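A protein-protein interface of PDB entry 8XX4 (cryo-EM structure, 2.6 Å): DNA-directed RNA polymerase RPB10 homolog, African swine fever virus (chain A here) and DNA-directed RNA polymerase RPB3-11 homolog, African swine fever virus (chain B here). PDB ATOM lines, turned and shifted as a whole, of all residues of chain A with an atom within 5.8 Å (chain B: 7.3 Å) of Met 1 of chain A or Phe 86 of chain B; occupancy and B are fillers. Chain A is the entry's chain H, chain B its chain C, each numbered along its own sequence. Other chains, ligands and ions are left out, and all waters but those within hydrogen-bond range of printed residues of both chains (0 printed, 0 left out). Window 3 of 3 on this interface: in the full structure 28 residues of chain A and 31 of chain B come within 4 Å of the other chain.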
ATOM      1  N   MET A   1     -19.171  23.789   7.392  1.00  0.00           N
ATOM      2  CA  MET A   1     -18.536  23.072   6.298  1.00  0.00           C
ATOM      3  C   MET A   1     -18.102  21.689   6.750  1.00  0.00           C
ATOM      4  O   MET A   1     -17.789  20.826   5.936  1.00  0.00           O
ATOM      5  CB  MET A   1     -17.341  23.855   5.768  1.00  0.00           C
ATOM      6  CG  MET A   1     -17.711  25.131   5.053  1.00  0.00           C
ATOM      7  SD  MET A   1     -16.276  25.950   4.359  1.00  0.00           S
ATOM      8  CE  MET A   1     -16.200  27.397   5.399  1.00  0.00           C
ATOM      9  N   LEU A   2     -18.084  21.490   8.063  1.00  0.00           N
ATOM     10  CA  LEU A   2     -17.726  20.225   8.681  1.00  0.00           C
ATOM     11  C   LEU A   2     -18.699  19.944   9.814  1.00  0.00           C
ATOM     12  O   LEU A   2     -19.511  20.792  10.183  1.00  0.00           O
ATOM     13  CB  LEU A   2     -16.290  20.244   9.219  1.00  0.00           C
ATOM     14  CG  LEU A   2     -15.153  20.446   8.224  1.00  0.00           C
ATOM     15  CD1 LEU A   2     -13.904  20.898   8.936  1.00  0.00           C
ATOM     16  CD2 LEU A   2     -14.899  19.164   7.473  1.00  0.00           C
ATOM     17  N   ILE A   3     -18.617  18.736  10.361  1.00  0.00           N
ATOM     18  CA  ILE A   3     -19.332  18.484  11.614  1.00  0.00           C
ATOM     19  C   ILE A   3     -18.778  19.420  12.677  1.00  0.00           C
ATOM     20  O   ILE A   3     -17.546  19.538  12.811  1.00  0.00           O
ATOM     21  CB  ILE A   3     -19.185  17.011  12.040  1.00  0.00           C
ATOM     22  CG1 ILE A   3     -20.029  16.113  11.145  1.00  0.00           C
ATOM     23  CG2 ILE A   3     -19.604  16.817  13.481  1.00  0.00           C
ATOM     24  CD1 ILE A   3     -19.532  14.702  11.066  1.00  0.00           C
ATOM     25  N   LEU A  74     -23.804  18.645   6.968  1.00  0.00           N
ATOM     26  CA  LEU A  74     -23.254  18.425   5.641  1.00  0.00           C
ATOM     27  C   LEU A  74     -21.757  18.677   5.641  1.00  0.00           C
ATOM     28  O   LEU A  74     -21.269  19.608   6.283  1.00  0.00           O
ATOM     29  CB  LEU A  74     -23.928  19.338   4.620  1.00  0.00           C
ATOM     30  CG  LEU A  74     -25.447  19.295   4.524  1.00  0.00           C
ATOM     31  CD1 LEU A  74     -25.931  20.408   3.626  1.00  0.00           C
ATOM     32  CD2 LEU A  74     -25.910  17.950   4.012  1.00  0.00           C
ATOM     33  N   ASP A  75     -21.030  17.842   4.913  1.00  0.00           N
ATOM     34  CA  ASP A  75     -19.594  17.986   4.753  1.00  0.00           C
ATOM     35  C   ASP A  75     -19.319  18.725   3.453  1.00  0.00           C
ATOM     36  O   ASP A  75     -19.744  18.282   2.384  1.00  0.00           O
ATOM     37  CB  ASP A  75     -18.912  16.620   4.746  1.00  0.00           C
ATOM     38  CG  ASP A  75     -17.444  16.697   5.085  1.00  0.00           C
ATOM     39  OD1 ASP A  75     -16.896  17.817   5.110  1.00  0.00           O
ATOM     40  OD2 ASP A  75     -16.832  15.638   5.324  1.00  0.00           O
ATOM     41  N   TYR A  76     -18.616  19.854   3.550  1.00  0.00           N
ATOM     42  CA  TYR A  76     -18.293  20.623   2.355  1.00  0.00           C
ATOM     43  C   TYR A  76     -17.410  19.832   1.405  1.00  0.00           C
ATOM     44  O   TYR A  76     -17.486  20.019   0.186  1.00  0.00           O
ATOM     45  CB  TYR A  76     -17.608  21.926   2.744  1.00  0.00           C
ATOM     46  CG  TYR A  76     -17.776  23.035   1.741  1.00  0.00           C
ATOM     47  CD1 TYR A  76     -18.969  23.730   1.645  1.00  0.00           C
ATOM     48  CD2 TYR A  76     -16.740  23.392   0.893  1.00  0.00           C
ATOM     49  CE1 TYR A  76     -19.126  24.745   0.733  1.00  0.00           C
ATOM     50  CE2 TYR A  76     -16.890  24.407  -0.021  1.00  0.00           C
ATOM     51  CZ  TYR A  76     -18.084  25.078  -0.096  1.00  0.00           C
ATOM     52  OH  TYR A  76     -18.240  26.094  -1.005  1.00  0.00           O
ATOM     53  N   ARG A  77     -16.567  18.952   1.937  1.00  0.00           N
ATOM     54  CA  ARG A  77     -15.682  18.169   1.087  1.00  0.00           C
ATOM     55  C   ARG A  77     -16.454  17.176   0.229  1.00  0.00           C
ATOM     56  O   ARG A  77     -15.988  16.804  -0.852  1.00  0.00           O
ATOM     57  CB  ARG A  77     -14.648  17.449   1.947  1.00  0.00           C
ATOM     58  CG  ARG A  77     -13.867  18.378   2.846  1.00  0.00           C
ATOM     59  CD  ARG A  77     -13.033  17.607   3.839  1.00  0.00           C
ATOM     60  NE  ARG A  77     -13.858  16.903   4.809  1.00  0.00           N
ATOM     61  CZ  ARG A  77     -13.416  16.439   5.968  1.00  0.00           C
ATOM     62  NH1 ARG A  77     -12.157  16.592   6.337  1.00  0.00           N
ATOM     63  NH2 ARG A  77     -14.257  15.805   6.775  1.00  0.00           N
ATOM     64  N   TYR A  80     -18.001  19.997  -2.501  1.00  0.00           N
ATOM     65  CA  TYR A  80     -17.034  20.717  -3.311  1.00  0.00           C
ATOM     66  C   TYR A  80     -15.904  19.796  -3.741  1.00  0.00           C
ATOM     67  O   TYR A  80     -15.248  19.169  -2.914  1.00  0.00           O
ATOM     68  CB  TYR A  80     -16.470  21.909  -2.550  1.00  0.00           C
ATOM     69  CG  TYR A  80     -15.863  22.954  -3.448  1.00  0.00           C
ATOM     70  CD1 TYR A  80     -16.645  23.662  -4.343  1.00  0.00           C
ATOM     71  CD2 TYR A  80     -14.505  23.227  -3.407  1.00  0.00           C
ATOM     72  CE1 TYR A  80     -16.094  24.611  -5.169  1.00  0.00           C
ATOM     73  CE2 TYR A  80     -13.947  24.174  -4.228  1.00  0.00           C
ATOM     74  CZ  TYR A  80     -14.746  24.866  -5.105  1.00  0.00           C
ATOM     75  OH  TYR A  80     -14.200  25.818  -5.930  1.00  0.00           O
ATOM     76  OXT TYR A  80     -15.612  19.662  -4.926  1.00  0.00           O
ATOM     77  N   TYR B  77      -3.607  34.816  12.384  1.00  0.00           N
ATOM     78  CA  TYR B  77      -3.987  34.203  11.117  1.00  0.00           C
ATOM     79  C   TYR B  77      -3.227  34.895   9.995  1.00  0.00           C
ATOM     80  O   TYR B  77      -3.465  36.072   9.708  1.00  0.00           O
ATOM     81  CB  TYR B  77      -5.494  34.318  10.917  1.00  0.00           C
ATOM     82  CG  TYR B  77      -6.045  33.539   9.749  1.00  0.00           C
ATOM     83  CD1 TYR B  77      -6.043  34.071   8.470  1.00  0.00           C
ATOM     84  CD2 TYR B  77      -6.590  32.280   9.930  1.00  0.00           C
ATOM     85  CE1 TYR B  77      -6.552  33.367   7.405  1.00  0.00           C
ATOM     86  CE2 TYR B  77      -7.102  31.570   8.874  1.00  0.00           C
ATOM     87  CZ  TYR B  77      -7.080  32.117   7.613  1.00  0.00           C
ATOM     88  OH  TYR B  77      -7.593  31.404   6.556  1.00  0.00           O
ATOM     89  N   THR B  83      -2.692  30.830   1.062  1.00  0.00           N
ATOM     90  CA  THR B  83      -3.609  30.318   2.068  1.00  0.00           C
ATOM     91  C   THR B  83      -4.913  29.868   1.429  1.00  0.00           C
ATOM     92  O   THR B  83      -5.333  30.380   0.390  1.00  0.00           O
ATOM     93  CB  THR B  83      -3.888  31.373   3.136  1.00  0.00           C
ATOM     94  OG1 THR B  83      -4.207  32.619   2.511  1.00  0.00           O
ATOM     95  CG2 THR B  83      -2.678  31.549   4.032  1.00  0.00           C
ATOM     96  N   ASP B  84      -5.547  28.884   2.059  1.00  0.00           N
ATOM     97  CA  ASP B  84      -6.827  28.395   1.574  1.00  0.00           C
ATOM     98  C   ASP B  84      -7.874  29.495   1.657  1.00  0.00           C
ATOM     99  O   ASP B  84      -7.988  30.191   2.668  1.00  0.00           O
ATOM    100  CB  ASP B  84      -7.273  27.179   2.379  1.00  0.00           C
ATOM    101  CG  ASP B  84      -8.339  26.380   1.669  1.00  0.00           C
ATOM    102  OD1 ASP B  84      -8.506  26.573   0.451  1.00  0.00           O
ATOM    103  OD2 ASP B  84      -9.012  25.559   2.321  1.00  0.00           O
ATOM    104  N   LEU B  85      -8.635  29.655   0.578  1.00  0.00           N
ATOM    105  CA  LEU B  85      -9.659  30.685   0.529  1.00  0.00           C
ATOM    106  C   LEU B  85     -10.960  30.251   1.184  1.00  0.00           C
ATOM    107  O   LEU B  85     -11.791  31.106   1.504  1.00  0.00           O
ATOM    108  CB  LEU B  85      -9.912  31.081  -0.923  1.00  0.00           C
ATOM    109  CG  LEU B  85      -8.662  31.384  -1.745  1.00  0.00           C
ATOM    110  CD1 LEU B  85      -8.908  31.076  -3.201  1.00  0.00           C
ATOM    111  CD2 LEU B  85      -8.254  32.831  -1.564  1.00  0.00           C
ATOM    112  N   PHE B  86     -11.151  28.951   1.396  1.00  0.00           N
ATOM    113  CA  PHE B  86     -12.352  28.451   2.048  1.00  0.00           C
ATOM    114  C   PHE B  86     -12.218  28.398   3.560  1.00  0.00           C
ATOM    115  O   PHE B  86     -13.223  28.517   4.267  1.00  0.00           O
ATOM    116  CB  PHE B  86     -12.698  27.060   1.519  1.00  0.00           C
ATOM    117  CG  PHE B  86     -13.207  27.062   0.113  1.00  0.00           C
ATOM    118  CD1 PHE B  86     -14.552  27.206  -0.148  1.00  0.00           C
ATOM    119  CD2 PHE B  86     -12.336  26.927  -0.950  1.00  0.00           C
ATOM    120  CE1 PHE B  86     -15.021  27.212  -1.439  1.00  0.00           C
ATOM    121  CE2 PHE B  86     -12.801  26.933  -2.244  1.00  0.00           C
ATOM    122  CZ  PHE B  86     -14.146  27.077  -2.485  1.00  0.00           C
ATOM    123  N   MET B  87     -11.001  28.222   4.071  1.00  0.00           N
ATOM    124  CA  MET B  87     -10.759  28.200   5.512  1.00  0.00           C
ATOM    125  C   MET B  87     -10.534  29.632   5.979  1.00  0.00           C
ATOM    126  O   MET B  87      -9.410  30.084   6.199  1.00  0.00           O
ATOM    127  CB  MET B  87      -9.574  27.302   5.844  1.00  0.00           C
ATOM    128  CG  MET B  87      -9.796  25.844   5.509  1.00  0.00           C
ATOM    129  SD  MET B  87     -11.141  25.089   6.435  1.00  0.00           S
ATOM    130  CE  MET B  87     -12.407  24.990   5.184  1.00  0.00           C
ATOM    131  N   THR B  88     -11.637  30.357   6.126  1.00  0.00           N
ATOM    132  CA  THR B  88     -11.554  31.746   6.536  1.00  0.00           C
ATOM    133  C   THR B  88     -11.141  31.842   7.998  1.00  0.00           C
ATOM    134  O   THR B  88     -11.183  30.867   8.749  1.00  0.00           O
ATOM    135  CB  THR B  88     -12.887  32.456   6.316  1.00  0.00           C
ATOM    136  OG1 THR B  88     -13.841  31.996   7.277  1.00  0.00           O
ATOM    137  CG2 THR B  88     -13.412  32.168   4.931  1.00  0.00           C
ATOM    138  N   GLU B  89     -10.719  33.042   8.395  1.00  0.00           N
ATOM    139  CA  GLU B  89     -10.298  33.252   9.775  1.00  0.00           C
ATOM    140  C   GLU B  89     -11.445  33.019  10.743  1.00  0.00           C
ATOM    141  O   GLU B  89     -11.251  32.436  11.812  1.00  0.00           O
ATOM    142  CB  GLU B  89      -9.741  34.660   9.948  1.00  0.00           C
ATOM    143  CG  GLU B  89      -9.216  34.932  11.341  1.00  0.00           C
ATOM    144  CD  GLU B  89      -8.370  36.177  11.411  1.00  0.00           C
ATOM    145  OE1 GLU B  89      -8.458  37.010  10.486  1.00  0.00           O
ATOM    146  OE2 GLU B  89      -7.619  36.327  12.395  1.00  0.00           O
ATOM    147  N   PHE B  91     -14.234  31.129  10.411  1.00  0.00           N
ATOM    148  CA  PHE B  91     -14.580  29.715  10.506  1.00  0.00           C
ATOM    149  C   PHE B  91     -13.565  28.956  11.353  1.00  0.00           C
ATOM    150  O   PHE B  91     -13.931  28.227  12.281  1.00  0.00           O
ATOM    151  CB  PHE B  91     -14.669  29.118   9.101  1.00  0.00           C
ATOM    152  CG  PHE B  91     -15.009  27.658   9.076  1.00  0.00           C
ATOM    153  CD1 PHE B  91     -16.294  27.229   9.343  1.00  0.00           C
ATOM    154  CD2 PHE B  91     -14.046  26.715   8.776  1.00  0.00           C
ATOM    155  CE1 PHE B  91     -16.608  25.897   9.319  1.00  0.00           C
ATOM    156  CE2 PHE B  91     -14.359  25.380   8.753  1.00  0.00           C
ATOM    157  CZ  PHE B  91     -15.641  24.971   9.025  1.00  0.00           C
ATOM    158  N   ILE B  92     -12.278  29.141  11.060  1.00  0.00           N
ATOM    159  CA  ILE B  92     -11.232  28.413  11.768  1.00  0.00           C
ATOM    160  C   ILE B  92     -11.163  28.849  13.224  1.00  0.00           C
ATOM    161  O   ILE B  92     -10.918  28.034  14.118  1.00  0.00           O
ATOM    162  CB  ILE B  92      -9.881  28.600  11.058  1.00  0.00           C
ATOM    163  CG1 ILE B  92      -9.934  28.001   9.658  1.00  0.00           C
ATOM    164  CG2 ILE B  92      -8.780  27.947  11.848  1.00  0.00           C
ATOM    165  CD1 ILE B  92     -10.145  26.519   9.647  1.00  0.00           C
ATOM    166  N   ARG B  95     -13.823  27.070  15.011  1.00  0.00           N
ATOM    167  CA  ARG B  95     -13.436  25.681  15.260  1.00  0.00           C
ATOM    168  C   ARG B  95     -12.473  25.582  16.436  1.00  0.00           C
ATOM    169  O   ARG B  95     -12.613  24.710  17.299  1.00  0.00           O
ATOM    170  CB  ARG B  95     -12.793  25.058  14.020  1.00  0.00           C
ATOM    171  CG  ARG B  95     -13.479  25.321  12.713  1.00  0.00           C
ATOM    172  CD  ARG B  95     -14.595  24.356  12.453  1.00  0.00           C
ATOM    173  NE  ARG B  95     -14.190  22.969  12.613  1.00  0.00           N
ATOM    174  CZ  ARG B  95     -15.029  21.947  12.563  1.00  0.00           C
ATOM    175  NH1 ARG B  95     -16.322  22.127  12.360  1.00  0.00           N
ATOM    176  NH2 ARG B  95     -14.561  20.715  12.725  1.00  0.00           N
ATOM    177  N   GLU B 147     -11.288  18.011  13.584  1.00  0.00           N
ATOM    178  CA  GLU B 147     -11.031  18.497  12.232  1.00  0.00           C
ATOM    179  C   GLU B 147     -11.045  20.016  12.279  1.00  0.00           C
ATOM    180  O   GLU B 147     -12.107  20.638  12.312  1.00  0.00           O
ATOM    181  CB  GLU B 147     -12.063  17.964  11.248  1.00  0.00           C
ATOM    182  CG  GLU B 147     -12.253  16.471  11.283  1.00  0.00           C
ATOM    183  CD  GLU B 147     -13.361  16.017  10.362  1.00  0.00           C
ATOM    184  OE1 GLU B 147     -14.515  16.452  10.557  1.00  0.00           O
ATOM    185  OE2 GLU B 147     -13.079  15.226   9.441  1.00  0.00           O
ATOM    186  N   PHE B 150     -10.041  21.809   6.230  1.00  0.00           N
ATOM    187  CA  PHE B 150      -9.519  21.085   5.084  1.00  0.00           C
ATOM    188  C   PHE B 150      -8.890  22.069   4.114  1.00  0.00           C
ATOM    189  O   PHE B 150      -9.408  23.167   3.905  1.00  0.00           O
ATOM    190  CB  PHE B 150     -10.613  20.271   4.386  1.00  0.00           C
ATOM    191  CG  PHE B 150     -11.859  21.048   4.086  1.00  0.00           C
ATOM    192  CD1 PHE B 150     -12.005  21.711   2.885  1.00  0.00           C
ATOM    193  CD2 PHE B 150     -12.893  21.102   5.000  1.00  0.00           C
ATOM    194  CE1 PHE B 150     -13.148  22.422   2.611  1.00  0.00           C
ATOM    195  CE2 PHE B 150     -14.039  21.812   4.725  1.00  0.00           C
ATOM    196  CZ  PHE B 150     -14.166  22.470   3.530  1.00  0.00           C
ATOM    197  N   GLN B 152      -7.559  23.028   0.317  1.00  0.00           N
ATOM    198  CA  GLN B 152      -7.594  22.758  -1.105  1.00  0.00           C
ATOM    199  C   GLN B 152      -6.177  22.474  -1.598  1.00  0.00           C
ATOM    200  O   GLN B 152      -5.202  22.912  -0.985  1.00  0.00           O
ATOM    201  CB  GLN B 152      -8.196  23.941  -1.856  1.00  0.00           C
ATOM    202  CG  GLN B 152      -9.653  24.208  -1.535  1.00  0.00           C
ATOM    203  CD  GLN B 152     -10.528  22.989  -1.727  1.00  0.00           C
ATOM    204  OE1 GLN B 152     -10.427  22.290  -2.732  1.00  0.00           O
ATOM    205  NE2 GLN B 152     -11.399  22.730  -0.764  1.00  0.00           N
ATOM    206  N   LYS B 155      -2.754  24.661  -1.261  1.00  0.00           N
ATOM    207  CA  LYS B 155      -3.042  25.743  -0.334  1.00  0.00           C
ATOM    208  C   LYS B 155      -2.465  25.439   1.041  1.00  0.00           C
ATOM    209  O   LYS B 155      -2.061  24.317   1.347  1.00  0.00           O
ATOM    210  CB  LYS B 155      -4.550  25.984  -0.241  1.00  0.00           C
ATOM    211  CG  LYS B 155      -5.184  26.443  -1.535  1.00  0.00           C
ATOM    212  CD  LYS B 155      -4.373  27.540  -2.180  1.00  0.00           C
ATOM    213  CE  LYS B 155      -5.198  28.310  -3.191  1.00  0.00           C
ATOM    214  NZ  LYS B 155      -4.877  29.762  -3.163  1.00  0.00           N
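Of chain A, only Met 1, Tyr 76 and Tyr 80 come within 4 Å of Phe 86 of chain B. Of the printed residues of chain A, Phe 91 of chain B touches Met 1 (3.8 Å). Of the printed residues of chain A, Phe 150 of chain B touches Leu 2, Tyr 76 and Arg 77. Gln 152 of chain B touches none of the printed residues of chain A. The nearest printed residue of chain A that does not touch Phe 86 of chain B is Arg 77 of chain A (8.7 Å).
The guanidinium group (NH2) of Arg 77 of chain A lies within salt-bridge range of the side-chain carboxylate (OD2) of Asp 75 of chain A (3.0 Å). SD of Met 87 of chain B lies within hydrogen-bond range of N of Phe 150 of chain B, at 3.5 Å. OG1 of Thr 88 of chain B lies within hydrogen-bond range of N of Phe 91 of chain B, 3.3 Å away. O of Met 1 of chain A lies within hydrogen-bond range of N of Tyr 76 of chain A (2.7 Å). The backbone carbonyl oxygen of Glu 147 of chain B sits at hydrogen-bond distance from the guanidinium group of Arg 95 of chain B, 2.5 Å away.
Hydrophobic or aromatic side chains of chain A that line the printed part of chain B: Met 1, Leu 2, Tyr 76 and Tyr 80. Along chain A the printed residues that touch a printed residue of chain B span positions 1 to 80. Among the printed residues, 11 pairs touch across the chains. Among the printed residues, Asp or Glu carboxylates within 4 Å of a Lys or Arg side-chain nitrogen of the other chain: Arg 77 of chain A with Glu 147 of chain B.
Phe 86 of chain B touches Met 1 of chain A. Met 1 of chain A touches Phe 91 of chain B. Leu 2 of chain A touches Arg 95 of chain B (CB to NH1, 3.7 Å). Glu 147 of chain B touches Leu 2 of chain A. Leu 2 of chain A touches Phe 150 of chain B (CD2 to CD2, 3.7 Å). Tyr 76 of chain A touches Phe 86 of chain B. CB of Tyr 76 of chain A touches CZ of Phe 150 of chain B, at 3.6 Å. Phe 150 of chain B touches Arg 77 of chain A. Tyr 80 of chain A touches Phe 86 of chain B.
The guanidinium group (NH2) of Arg 77 of chain A lies within salt-bridge range of the side-chain carboxylate (OE2) of Glu 147 of chain B (3.0 Å). NH1 of Arg 95 of chain B lies within hydrogen-bond range of O of Ile 3 of chain A (2.9 Å).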
